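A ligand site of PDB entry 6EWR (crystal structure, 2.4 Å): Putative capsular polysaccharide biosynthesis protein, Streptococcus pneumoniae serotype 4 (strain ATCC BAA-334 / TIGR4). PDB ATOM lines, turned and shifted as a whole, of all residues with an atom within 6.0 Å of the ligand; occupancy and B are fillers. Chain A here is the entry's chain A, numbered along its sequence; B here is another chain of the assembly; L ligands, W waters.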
ATOM      1  N   ASN A  62     -13.609   6.769  16.943  1.00  0.00           N
ATOM      2  CA  ASN A  62     -12.688   7.788  17.488  1.00  0.00           C
ATOM      3  C   ASN A  62     -13.332   8.958  18.229  1.00  0.00           C
ATOM      4  O   ASN A  62     -12.599   9.740  18.835  1.00  0.00           O
ATOM      5  CB  ASN A  62     -11.705   8.345  16.416  1.00  0.00           C
ATOM      6  CG  ASN A  62     -12.393   9.177  15.320  1.00  0.00           C
ATOM      7  OD1 ASN A  62     -13.614   9.491  15.387  1.00  0.00           O
ATOM      8  ND2 ASN A  62     -11.621   9.537  14.311  1.00  0.00           N
ATOM      9  N   SER A  63     -14.657   9.086  18.155  1.00  0.00           N
ATOM     10  CA  SER A  63     -15.397  10.063  18.994  1.00  0.00           C
ATOM     11  C   SER A  63     -16.875   9.711  19.084  1.00  0.00           C
ATOM     12  O   SER A  63     -17.381   8.938  18.275  1.00  0.00           O
ATOM     13  CB  SER A  63     -15.247  11.477  18.421  1.00  0.00           C
ATOM     14  OG  SER A  63     -15.903  11.603  17.181  1.00  0.00           O
ATOM     15  N   ALA A  64     -17.584  10.306  20.049  1.00  0.00           N
ATOM     16  CA  ALA A  64     -19.070  10.237  20.072  1.00  0.00           C
ATOM     17  C   ALA A  64     -19.665  11.017  18.930  1.00  0.00           C
ATOM     18  O   ALA A  64     -20.751  10.698  18.437  1.00  0.00           O
ATOM     19  CB  ALA A  64     -19.603  10.788  21.403  1.00  0.00           C
ATOM     20  N   THR A  65     -18.980  12.107  18.553  1.00  0.00           N
ATOM     21  CA  THR A  65     -19.386  12.931  17.414  1.00  0.00           C
ATOM     22  C   THR A  65     -19.345  12.110  16.131  1.00  0.00           C
ATOM     23  O   THR A  65     -20.291  12.215  15.336  1.00  0.00           O
ATOM     24  CB  THR A  65     -18.487  14.184  17.291  1.00  0.00           C
ATOM     25  OG1 THR A  65     -18.586  14.949  18.516  1.00  0.00           O
ATOM     26  CG2 THR A  65     -18.941  15.037  16.106  1.00  0.00           C
ATOM     27  N   ALA A  66     -18.287  11.285  15.952  1.00  0.00           N
ATOM     28  CA  ALA A  66     -18.260  10.315  14.863  1.00  0.00           C
ATOM     29  C   ALA A  66     -19.425   9.297  14.922  1.00  0.00           C
ATOM     30  O   ALA A  66     -20.108   9.024  13.908  1.00  0.00           O
ATOM     31  CB  ALA A  66     -16.934   9.577  14.834  1.00  0.00           C
ATOM     32  N   LEU A  68     -22.350   9.562  16.553  1.00  0.00           N
ATOM     33  CA  LEU A  68     -23.639  10.210  16.410  1.00  0.00           C
ATOM     34  C   LEU A  68     -23.882  10.525  14.925  1.00  0.00           C
ATOM     35  O   LEU A  68     -24.942  10.203  14.402  1.00  0.00           O
ATOM     36  CB  LEU A  68     -23.711  11.475  17.289  1.00  0.00           C
ATOM     37  CG  LEU A  68     -25.087  12.096  17.530  1.00  0.00           C
ATOM     38  CD1 LEU A  68     -26.117  11.099  18.046  1.00  0.00           C
ATOM     39  CD2 LEU A  68     -25.032  13.308  18.462  1.00  0.00           C
ATOM     40  N   THR A  89     -27.788  21.879  25.429  1.00  0.00           N
ATOM     41  CA  THR A  89     -26.863  20.779  25.243  1.00  0.00           C
ATOM     42  C   THR A  89     -25.568  21.308  24.685  1.00  0.00           C
ATOM     43  O   THR A  89     -25.474  22.498  24.358  1.00  0.00           O
ATOM     44  CB  THR A  89     -27.417  19.702  24.292  1.00  0.00           C
ATOM     45  OG1 THR A  89     -26.496  18.616  24.184  1.00  0.00           O
ATOM     46  CG2 THR A  89     -27.684  20.289  22.916  1.00  0.00           C
ATOM     47  N   TYR A  90     -24.584  20.415  24.609  1.00  0.00           N
ATOM     48  CA  TYR A  90     -23.316  20.690  23.948  1.00  0.00           C
ATOM     49  C   TYR A  90     -23.511  20.724  22.419  1.00  0.00           C
ATOM     50  O   TYR A  90     -24.350  19.993  21.858  1.00  0.00           O
ATOM     51  CB  TYR A  90     -22.266  19.625  24.304  1.00  0.00           C
ATOM     52  CG  TYR A  90     -20.851  19.987  23.900  1.00  0.00           C
ATOM     53  CD1 TYR A  90     -20.251  21.120  24.413  1.00  0.00           C
ATOM     54  CD2 TYR A  90     -20.125  19.206  23.025  1.00  0.00           C
ATOM     55  CE1 TYR A  90     -18.959  21.465  24.076  1.00  0.00           C
ATOM     56  CE2 TYR A  90     -18.829  19.555  22.651  1.00  0.00           C
ATOM     57  CZ  TYR A  90     -18.255  20.692  23.194  1.00  0.00           C
ATOM     58  OH  TYR A  90     -16.949  21.097  22.903  1.00  0.00           O
ATOM     59  N   ALA A  92     -21.858  19.502  19.933  1.00  0.00           N
ATOM     60  CA  ALA A  92     -21.701  18.215  19.241  1.00  0.00           C
ATOM     61  C   ALA A  92     -23.027  17.450  19.016  1.00  0.00           C
ATOM     62  O   ALA A  92     -23.149  16.723  18.034  1.00  0.00           O
ATOM     63  CB  ALA A  92     -20.709  17.347  19.967  1.00  0.00           C
ATOM     64  N   SER A  93     -23.993  17.617  19.910  1.00  0.00           N
ATOM     65  CA  SER A  93     -25.326  17.012  19.728  1.00  0.00           C
ATOM     66  C   SER A  93     -25.986  17.528  18.452  1.00  0.00           C
ATOM     67  O   SER A  93     -26.681  16.770  17.795  1.00  0.00           O
ATOM     68  CB  SER A  93     -26.274  17.325  20.918  1.00  0.00           C
ATOM     69  OG  SER A  93     -25.705  17.036  22.194  1.00  0.00           O
ATOM     70  N   VAL A 135     -30.523  14.216  25.121  1.00  0.00           N
ATOM     71  CA  VAL A 135     -29.176  14.149  25.693  1.00  0.00           C
ATOM     72  C   VAL A 135     -29.308  13.794  27.156  1.00  0.00           C
ATOM     73  O   VAL A 135     -30.055  14.426  27.894  1.00  0.00           O
ATOM     74  CB  VAL A 135     -28.363  15.451  25.486  1.00  0.00           C
ATOM     75  CG1 VAL A 135     -29.142  16.696  25.852  1.00  0.00           C
ATOM     76  CG2 VAL A 135     -27.060  15.423  26.284  1.00  0.00           C
ATOM     77  N   LEU A 137     -27.907  14.372  29.968  1.00  0.00           N
ATOM     78  CA  LEU A 137     -27.036  15.359  30.580  1.00  0.00           C
ATOM     79  C   LEU A 137     -26.609  14.971  31.982  1.00  0.00           C
ATOM     80  O   LEU A 137     -27.461  14.711  32.841  1.00  0.00           O
ATOM     81  CB  LEU A 137     -27.754  16.700  30.666  1.00  0.00           C
ATOM     82  CG  LEU A 137     -26.931  17.850  31.242  1.00  0.00           C
ATOM     83  CD1 LEU A 137     -26.077  18.439  30.172  1.00  0.00           C
ATOM     84  CD2 LEU A 137     -27.815  18.942  31.816  1.00  0.00           C
ATOM     85  N   ASP A 176     -28.067  10.839  22.695  1.00  0.00           N
ATOM     86  CA  ASP A 176     -26.724  11.371  22.976  1.00  0.00           C
ATOM     87  C   ASP A 176     -26.308  10.968  24.411  1.00  0.00           C
ATOM     88  O   ASP A 176     -26.516  11.740  25.374  1.00  0.00           O
ATOM     89  CB  ASP A 176     -26.682  12.887  22.779  1.00  0.00           C
ATOM     90  CG  ASP A 176     -25.256  13.466  22.953  1.00  0.00           C
ATOM     91  OD1 ASP A 176     -24.346  12.762  23.437  1.00  0.00           O
ATOM     92  OD2 ASP A 176     -25.041  14.632  22.617  1.00  0.00           O
ATOM     93  N   ALA A 178     -23.300  10.690  25.651  1.00  0.00           N
ATOM     94  CA  ALA A 178     -21.895  11.001  25.811  1.00  0.00           C
ATOM     95  C   ALA A 178     -21.465  10.880  27.279  1.00  0.00           C
ATOM     96  O   ALA A 178     -20.370  10.437  27.561  1.00  0.00           O
ATOM     97  CB  ALA A 178     -21.592  12.391  25.270  1.00  0.00           C
ATOM     98  N   HIS A 179     -22.364  11.258  28.195  1.00  0.00           N
ATOM     99  CA  HIS A 179     -22.081  11.315  29.631  1.00  0.00           C
ATOM    100  C   HIS A 179     -22.561  10.066  30.400  1.00  0.00           C
ATOM    101  O   HIS A 179     -22.254   9.918  31.599  1.00  0.00           O
ATOM    102  CB  HIS A 179     -22.826  12.506  30.250  1.00  0.00           C
ATOM    103  CG  HIS A 179     -22.526  13.839  29.619  1.00  0.00           C
ATOM    104  ND1 HIS A 179     -23.312  14.948  29.860  1.00  0.00           N
ATOM    105  CD2 HIS A 179     -21.547  14.243  28.777  1.00  0.00           C
ATOM    106  CE1 HIS A 179     -22.804  15.988  29.222  1.00  0.00           C
ATOM    107  NE2 HIS A 179     -21.747  15.590  28.531  1.00  0.00           N
ATOM    108  N   PHE A 199     -21.893   6.943  22.596  1.00  0.00           N
ATOM    109  CA  PHE A 199     -21.099   7.153  23.838  1.00  0.00           C
ATOM    110  C   PHE A 199     -19.764   7.893  23.534  1.00  0.00           C
ATOM    111  O   PHE A 199     -19.211   7.776  22.452  1.00  0.00           O
ATOM    112  CB  PHE A 199     -20.805   5.789  24.521  1.00  0.00           C
ATOM    113  CG  PHE A 199     -22.024   5.126  25.151  1.00  0.00           C
ATOM    114  CD1 PHE A 199     -22.588   5.646  26.324  1.00  0.00           C
ATOM    115  CD2 PHE A 199     -22.606   3.985  24.588  1.00  0.00           C
ATOM    116  CE1 PHE A 199     -23.700   5.043  26.908  1.00  0.00           C
ATOM    117  CE2 PHE A 199     -23.725   3.382  25.179  1.00  0.00           C
ATOM    118  CZ  PHE A 199     -24.276   3.920  26.334  1.00  0.00           C
ATOM    119  N   SER A 200     -19.268   8.646  24.512  1.00  0.00           N
ATOM    120  CA  SER A 200     -17.957   9.334  24.435  1.00  0.00           C
ATOM    121  C   SER A 200     -17.037   8.743  25.480  1.00  0.00           C
ATOM    122  O   SER A 200     -17.434   8.558  26.631  1.00  0.00           O
ATOM    123  CB  SER A 200     -18.110  10.856  24.737  1.00  0.00           C
ATOM    124  OG  SER A 200     -16.885  11.560  24.553  1.00  0.00           O
ATOM    125  N   PHE A 201     -15.809   8.498  25.062  1.00  0.00           N
ATOM    126  CA  PHE A 201     -14.725   8.071  25.939  1.00  0.00           C
ATOM    127  C   PHE A 201     -13.610   9.147  25.937  1.00  0.00           C
ATOM    128  O   PHE A 201     -12.419   8.847  26.071  1.00  0.00           O
ATOM    129  CB  PHE A 201     -14.178   6.705  25.499  1.00  0.00           C
ATOM    130  CG  PHE A 201     -15.233   5.703  25.102  1.00  0.00           C
ATOM    131  CD1 PHE A 201     -16.434   5.566  25.820  1.00  0.00           C
ATOM    132  CD2 PHE A 201     -14.987   4.806  24.052  1.00  0.00           C
ATOM    133  CE1 PHE A 201     -17.376   4.606  25.438  1.00  0.00           C
ATOM    134  CE2 PHE A 201     -15.915   3.847  23.669  1.00  0.00           C
ATOM    135  CZ  PHE A 201     -17.121   3.766  24.363  1.00  0.00           C
ATOM    136  N   HIS A 202     -14.011  10.396  25.792  1.00  0.00           N
ATOM    137  CA  HIS A 202     -13.074  11.537  25.824  1.00  0.00           C
ATOM    138  C   HIS A 202     -12.393  11.640  27.194  1.00  0.00           C
ATOM    139  O   HIS A 202     -12.964  11.233  28.201  1.00  0.00           O
ATOM    140  CB  HIS A 202     -13.868  12.808  25.553  1.00  0.00           C
ATOM    141  CG  HIS A 202     -13.042  14.045  25.487  1.00  0.00           C
ATOM    142  ND1 HIS A 202     -12.773  14.826  26.595  1.00  0.00           N
ATOM    143  CD2 HIS A 202     -12.473  14.669  24.439  1.00  0.00           C
ATOM    144  CE1 HIS A 202     -12.042  15.869  26.224  1.00  0.00           C
ATOM    145  NE2 HIS A 202     -11.868  15.797  24.917  1.00  0.00           N
ATOM    146  N   LYS A 205     -14.424  12.393  30.327  1.00  0.00           N
ATOM    147  CA  LYS A 205     -15.579  11.520  30.675  1.00  0.00           C
ATOM    148  C   LYS A 205     -15.241  10.479  31.765  1.00  0.00           C
ATOM    149  O   LYS A 205     -14.071  10.299  32.123  1.00  0.00           O
ATOM    150  CB  LYS A 205     -16.210  10.833  29.433  1.00  0.00           C
ATOM    151  CG  LYS A 205     -16.698  11.760  28.330  1.00  0.00           C
ATOM    152  CD  LYS A 205     -17.571  12.905  28.800  1.00  0.00           C
ATOM    153  CE  LYS A 205     -18.013  13.848  27.655  1.00  0.00           C
ATOM    154  NZ  LYS A 205     -16.968  14.777  27.094  1.00  0.00           N
ATOM    155  N   GLU A 211      -9.297   9.919  23.540  1.00  0.00           N
ATOM    156  CA  GLU A 211     -10.338  10.215  22.541  1.00  0.00           C
ATOM    157  C   GLU A 211     -10.924   8.888  22.078  1.00  0.00           C
ATOM    158  O   GLU A 211     -10.181   7.905  21.823  1.00  0.00           O
ATOM    159  CB  GLU A 211      -9.771  10.931  21.333  1.00  0.00           C
ATOM    160  CG  GLU A 211      -9.230  12.324  21.613  1.00  0.00           C
ATOM    161  CD  GLU A 211     -10.292  13.379  21.829  1.00  0.00           C
ATOM    162  OE1 GLU A 211     -11.459  13.163  21.480  1.00  0.00           O
ATOM    163  OE2 GLU A 211      -9.936  14.446  22.346  1.00  0.00           O
ATOM    164  N   GLY A 212     -12.247   8.840  21.987  1.00  0.00           N
ATOM    165  CA  GLY A 212     -12.926   7.648  21.518  1.00  0.00           C
ATOM    166  C   GLY A 212     -14.410   7.702  21.769  1.00  0.00           C
ATOM    167  O   GLY A 212     -14.914   8.536  22.514  1.00  0.00           O
ATOM    168  N   GLY A 213     -15.131   6.793  21.135  1.00  0.00           N
ATOM    169  CA  GLY A 213     -16.541   6.680  21.392  1.00  0.00           C
ATOM    170  C   GLY A 213     -17.097   5.420  20.785  1.00  0.00           C
ATOM    171  O   GLY A 213     -16.343   4.617  20.222  1.00  0.00           O
ATOM    172  N   TYR A 351     -25.016  24.355  30.139  1.00  0.00           N
ATOM    173  CA  TYR A 351     -24.243  24.929  29.025  1.00  0.00           C
ATOM    174  C   TYR A 351     -24.805  26.285  28.682  1.00  0.00           C
ATOM    175  O   TYR A 351     -25.927  26.612  29.065  1.00  0.00           O
ATOM    176  CB  TYR A 351     -24.395  24.073  27.788  1.00  0.00           C
ATOM    177  CG  TYR A 351     -23.785  22.693  27.866  1.00  0.00           C
ATOM    178  CD1 TYR A 351     -22.427  22.497  27.612  1.00  0.00           C
ATOM    179  CD2 TYR A 351     -24.574  21.582  28.166  1.00  0.00           C
ATOM    180  CE1 TYR A 351     -21.876  21.228  27.651  1.00  0.00           C
ATOM    181  CE2 TYR A 351     -24.029  20.314  28.213  1.00  0.00           C
ATOM    182  CZ  TYR A 351     -22.686  20.130  27.971  1.00  0.00           C
ATOM    183  OH  TYR A 351     -22.161  18.865  28.040  1.00  0.00           O
ATOM    184  N   HIS B 238     -14.638  21.133  17.389  1.00  0.00           N
ATOM    185  CA  HIS B 238     -16.044  21.550  17.425  1.00  0.00           C
ATOM    186  C   HIS B 238     -16.351  23.025  17.190  1.00  0.00           C
ATOM    187  O   HIS B 238     -17.442  23.497  17.515  1.00  0.00           O
ATOM    188  CB  HIS B 238     -16.714  21.155  18.759  1.00  0.00           C
ATOM    189  CG  HIS B 238     -16.607  19.711  19.122  1.00  0.00           C
ATOM    190  ND1 HIS B 238     -17.278  18.693  18.491  1.00  0.00           N
ATOM    191  CD2 HIS B 238     -15.896  19.128  20.128  1.00  0.00           C
ATOM    192  CE1 HIS B 238     -16.954  17.535  19.055  1.00  0.00           C
ATOM    193  NE2 HIS B 238     -16.156  17.775  20.069  1.00  0.00           N
ATOM    194  N   LYS B 263     -14.335  16.922  14.732  1.00  0.00           N
ATOM    195  CA  LYS B 263     -13.659  16.353  15.881  1.00  0.00           C
ATOM    196  C   LYS B 263     -12.504  15.493  15.415  1.00  0.00           C
ATOM    197  O   LYS B 263     -12.641  14.301  15.298  1.00  0.00           O
ATOM    198  CB  LYS B 263     -14.641  15.581  16.777  1.00  0.00           C
ATOM    199  CG  LYS B 263     -14.069  15.058  18.110  1.00  0.00           C
ATOM    200  CD  LYS B 263     -13.398  16.169  18.919  1.00  0.00           C
ATOM    201  CE  LYS B 263     -13.066  15.717  20.338  1.00  0.00           C
ATOM    202  NZ  LYS B 263     -11.846  16.322  20.958  1.00  0.00           N
HETATM  203  N1  LIG L   1     -22.623  15.417  23.484  1.00  0.00           N
HETATM  204  C1  LIG L   1     -22.347  15.964  24.707  1.00  0.00           C
HETATM  205  C2  LIG L   1     -23.476  16.386  25.612  1.00  0.00           C
HETATM  206  C3  LIG L   1     -20.951  16.153  25.157  1.00  0.00           C
HETATM  207  O1  LIG L   1     -20.621  16.711  26.360  1.00  0.00           O
HETATM  208  C4  LIG L   1     -19.901  15.698  24.211  1.00  0.00           C
HETATM  209  C5  LIG L   1     -18.464  15.863  24.620  1.00  0.00           C
HETATM  210  N2  LIG L   1     -17.562  16.365  23.562  1.00  0.00           N
HETATM  211  C6  LIG L   1     -20.309  15.104  22.889  1.00  0.00           C
HETATM  212  C7  LIG L   1     -21.677  14.997  22.602  1.00  0.00           C
HETATM  213  C8  LIG L   1     -19.262  14.636  21.874  1.00  0.00           C
HETATM  214  O2  LIG L   1     -18.126  14.031  22.536  1.00  0.00           O
HETATM  215  P1  LIG L   1     -16.807  13.608  21.720  1.00  0.00           P
HETATM  216  O3  LIG L   1     -17.166  13.623  20.261  1.00  0.00           O
HETATM  217  O4  LIG L   1     -16.355  12.203  22.172  1.00  0.00           O
HETATM  218  O5  LIG L   1     -15.748  14.626  21.984  1.00  0.00           O
HETATM  219  O   HOH W   1     -19.512  18.724  27.928  1.00  0.00           O
HETATM  220  O   HOH W   2     -13.743  11.663  22.345  1.00  0.00           O
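N of Thr 65 lies close to OG of Ser 63, 3.4 Å away. The side-chain carboxylate (OD2) of Asp 176 is in hydrogen-bond range of the side-chain hydroxyl (OG) of Ser 93 (2.5 Å). OH of Tyr 351 lies close to NE2 of His 179 (3.3 Å). The side-chain carboxylate (OE2) of Glu 211 lies within salt-bridge range of the side-chain amino group (NZ) of Lys 263 of chain B, 3.0 Å away. The backbone carbonyl oxygen (O) of Tyr 90 lies within hydrogen-bond range of the side-chain hydroxyl (OG) of Ser 93, 3.3 Å away. The side-chain hydroxyl of Thr 89 is in hydrogen-bond range of the side-chain hydroxyl of Ser 93, at 2.7 Å. O of Gly 212 lies within hydrogen-bond range of N of Phe 201 (2.7 Å). The backbone NH (N) of Gly 212 lies within hydrogen-bond range of the backbone carbonyl oxygen (O) of Asn 62 (3.3 Å).
Merely in contact with the ligand: Lys 205 (3.1 Å), Lys 263 of chain B (3.3 Å), Ser 63 (3.4 Å), Tyr 90 (3.6 Å), Ala 92 (3.6 Å), Ala 178 (3.7 Å), His 238 of chain B (3.7 Å), Ser 93 (3.7 Å), Val 135 (3.8 Å) and Gly 212 (3.95 Å). Hydrophobic or aromatic side chains that line the ligand: Ala 64, Tyr 90, Ala 92, Val 135, Ala 178 and His 179. Along chain A the residues within 4 Å of the ligand span positions 63 to 351.
The side-chain hydroxyl (OG) of Ser 200 lies within hydrogen-bond range of an oxygen (O4) of the ligand (2.5 Å). O3 of the ligand is in hydrogen-bond range of N of Thr 65, 2.9 Å away. An oxygen (O3) of the ligand lies within hydrogen-bond range of the side-chain hydroxyl of Thr 65, 2.6 Å away. The side-chain carboxylate (OD2) of Asp 176 lies within hydrogen-bond range of a nitrogen (N1) of the ligand, at 2.7 Å. O1 of the ligand is in hydrogen-bond range of NE2 of His 179, at 2.7 Å. O4 of the ligand sits at hydrogen-bond distance from N of Ala 64 (3.1 Å). The side-chain hydroxyl of Tyr 351 lies within hydrogen-bond range of an oxygen (O1) of the ligand.
Water W2 lies within hydrogen-bond range of O4 of the ligand (2.7 Å), OE1 of Glu 211 (2.9 Å) and N of Gly 212 (3.2 Å). Water W1 bridges OH of Tyr 351 (2.7 Å) and O1 of the ligand (2.8 Å).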
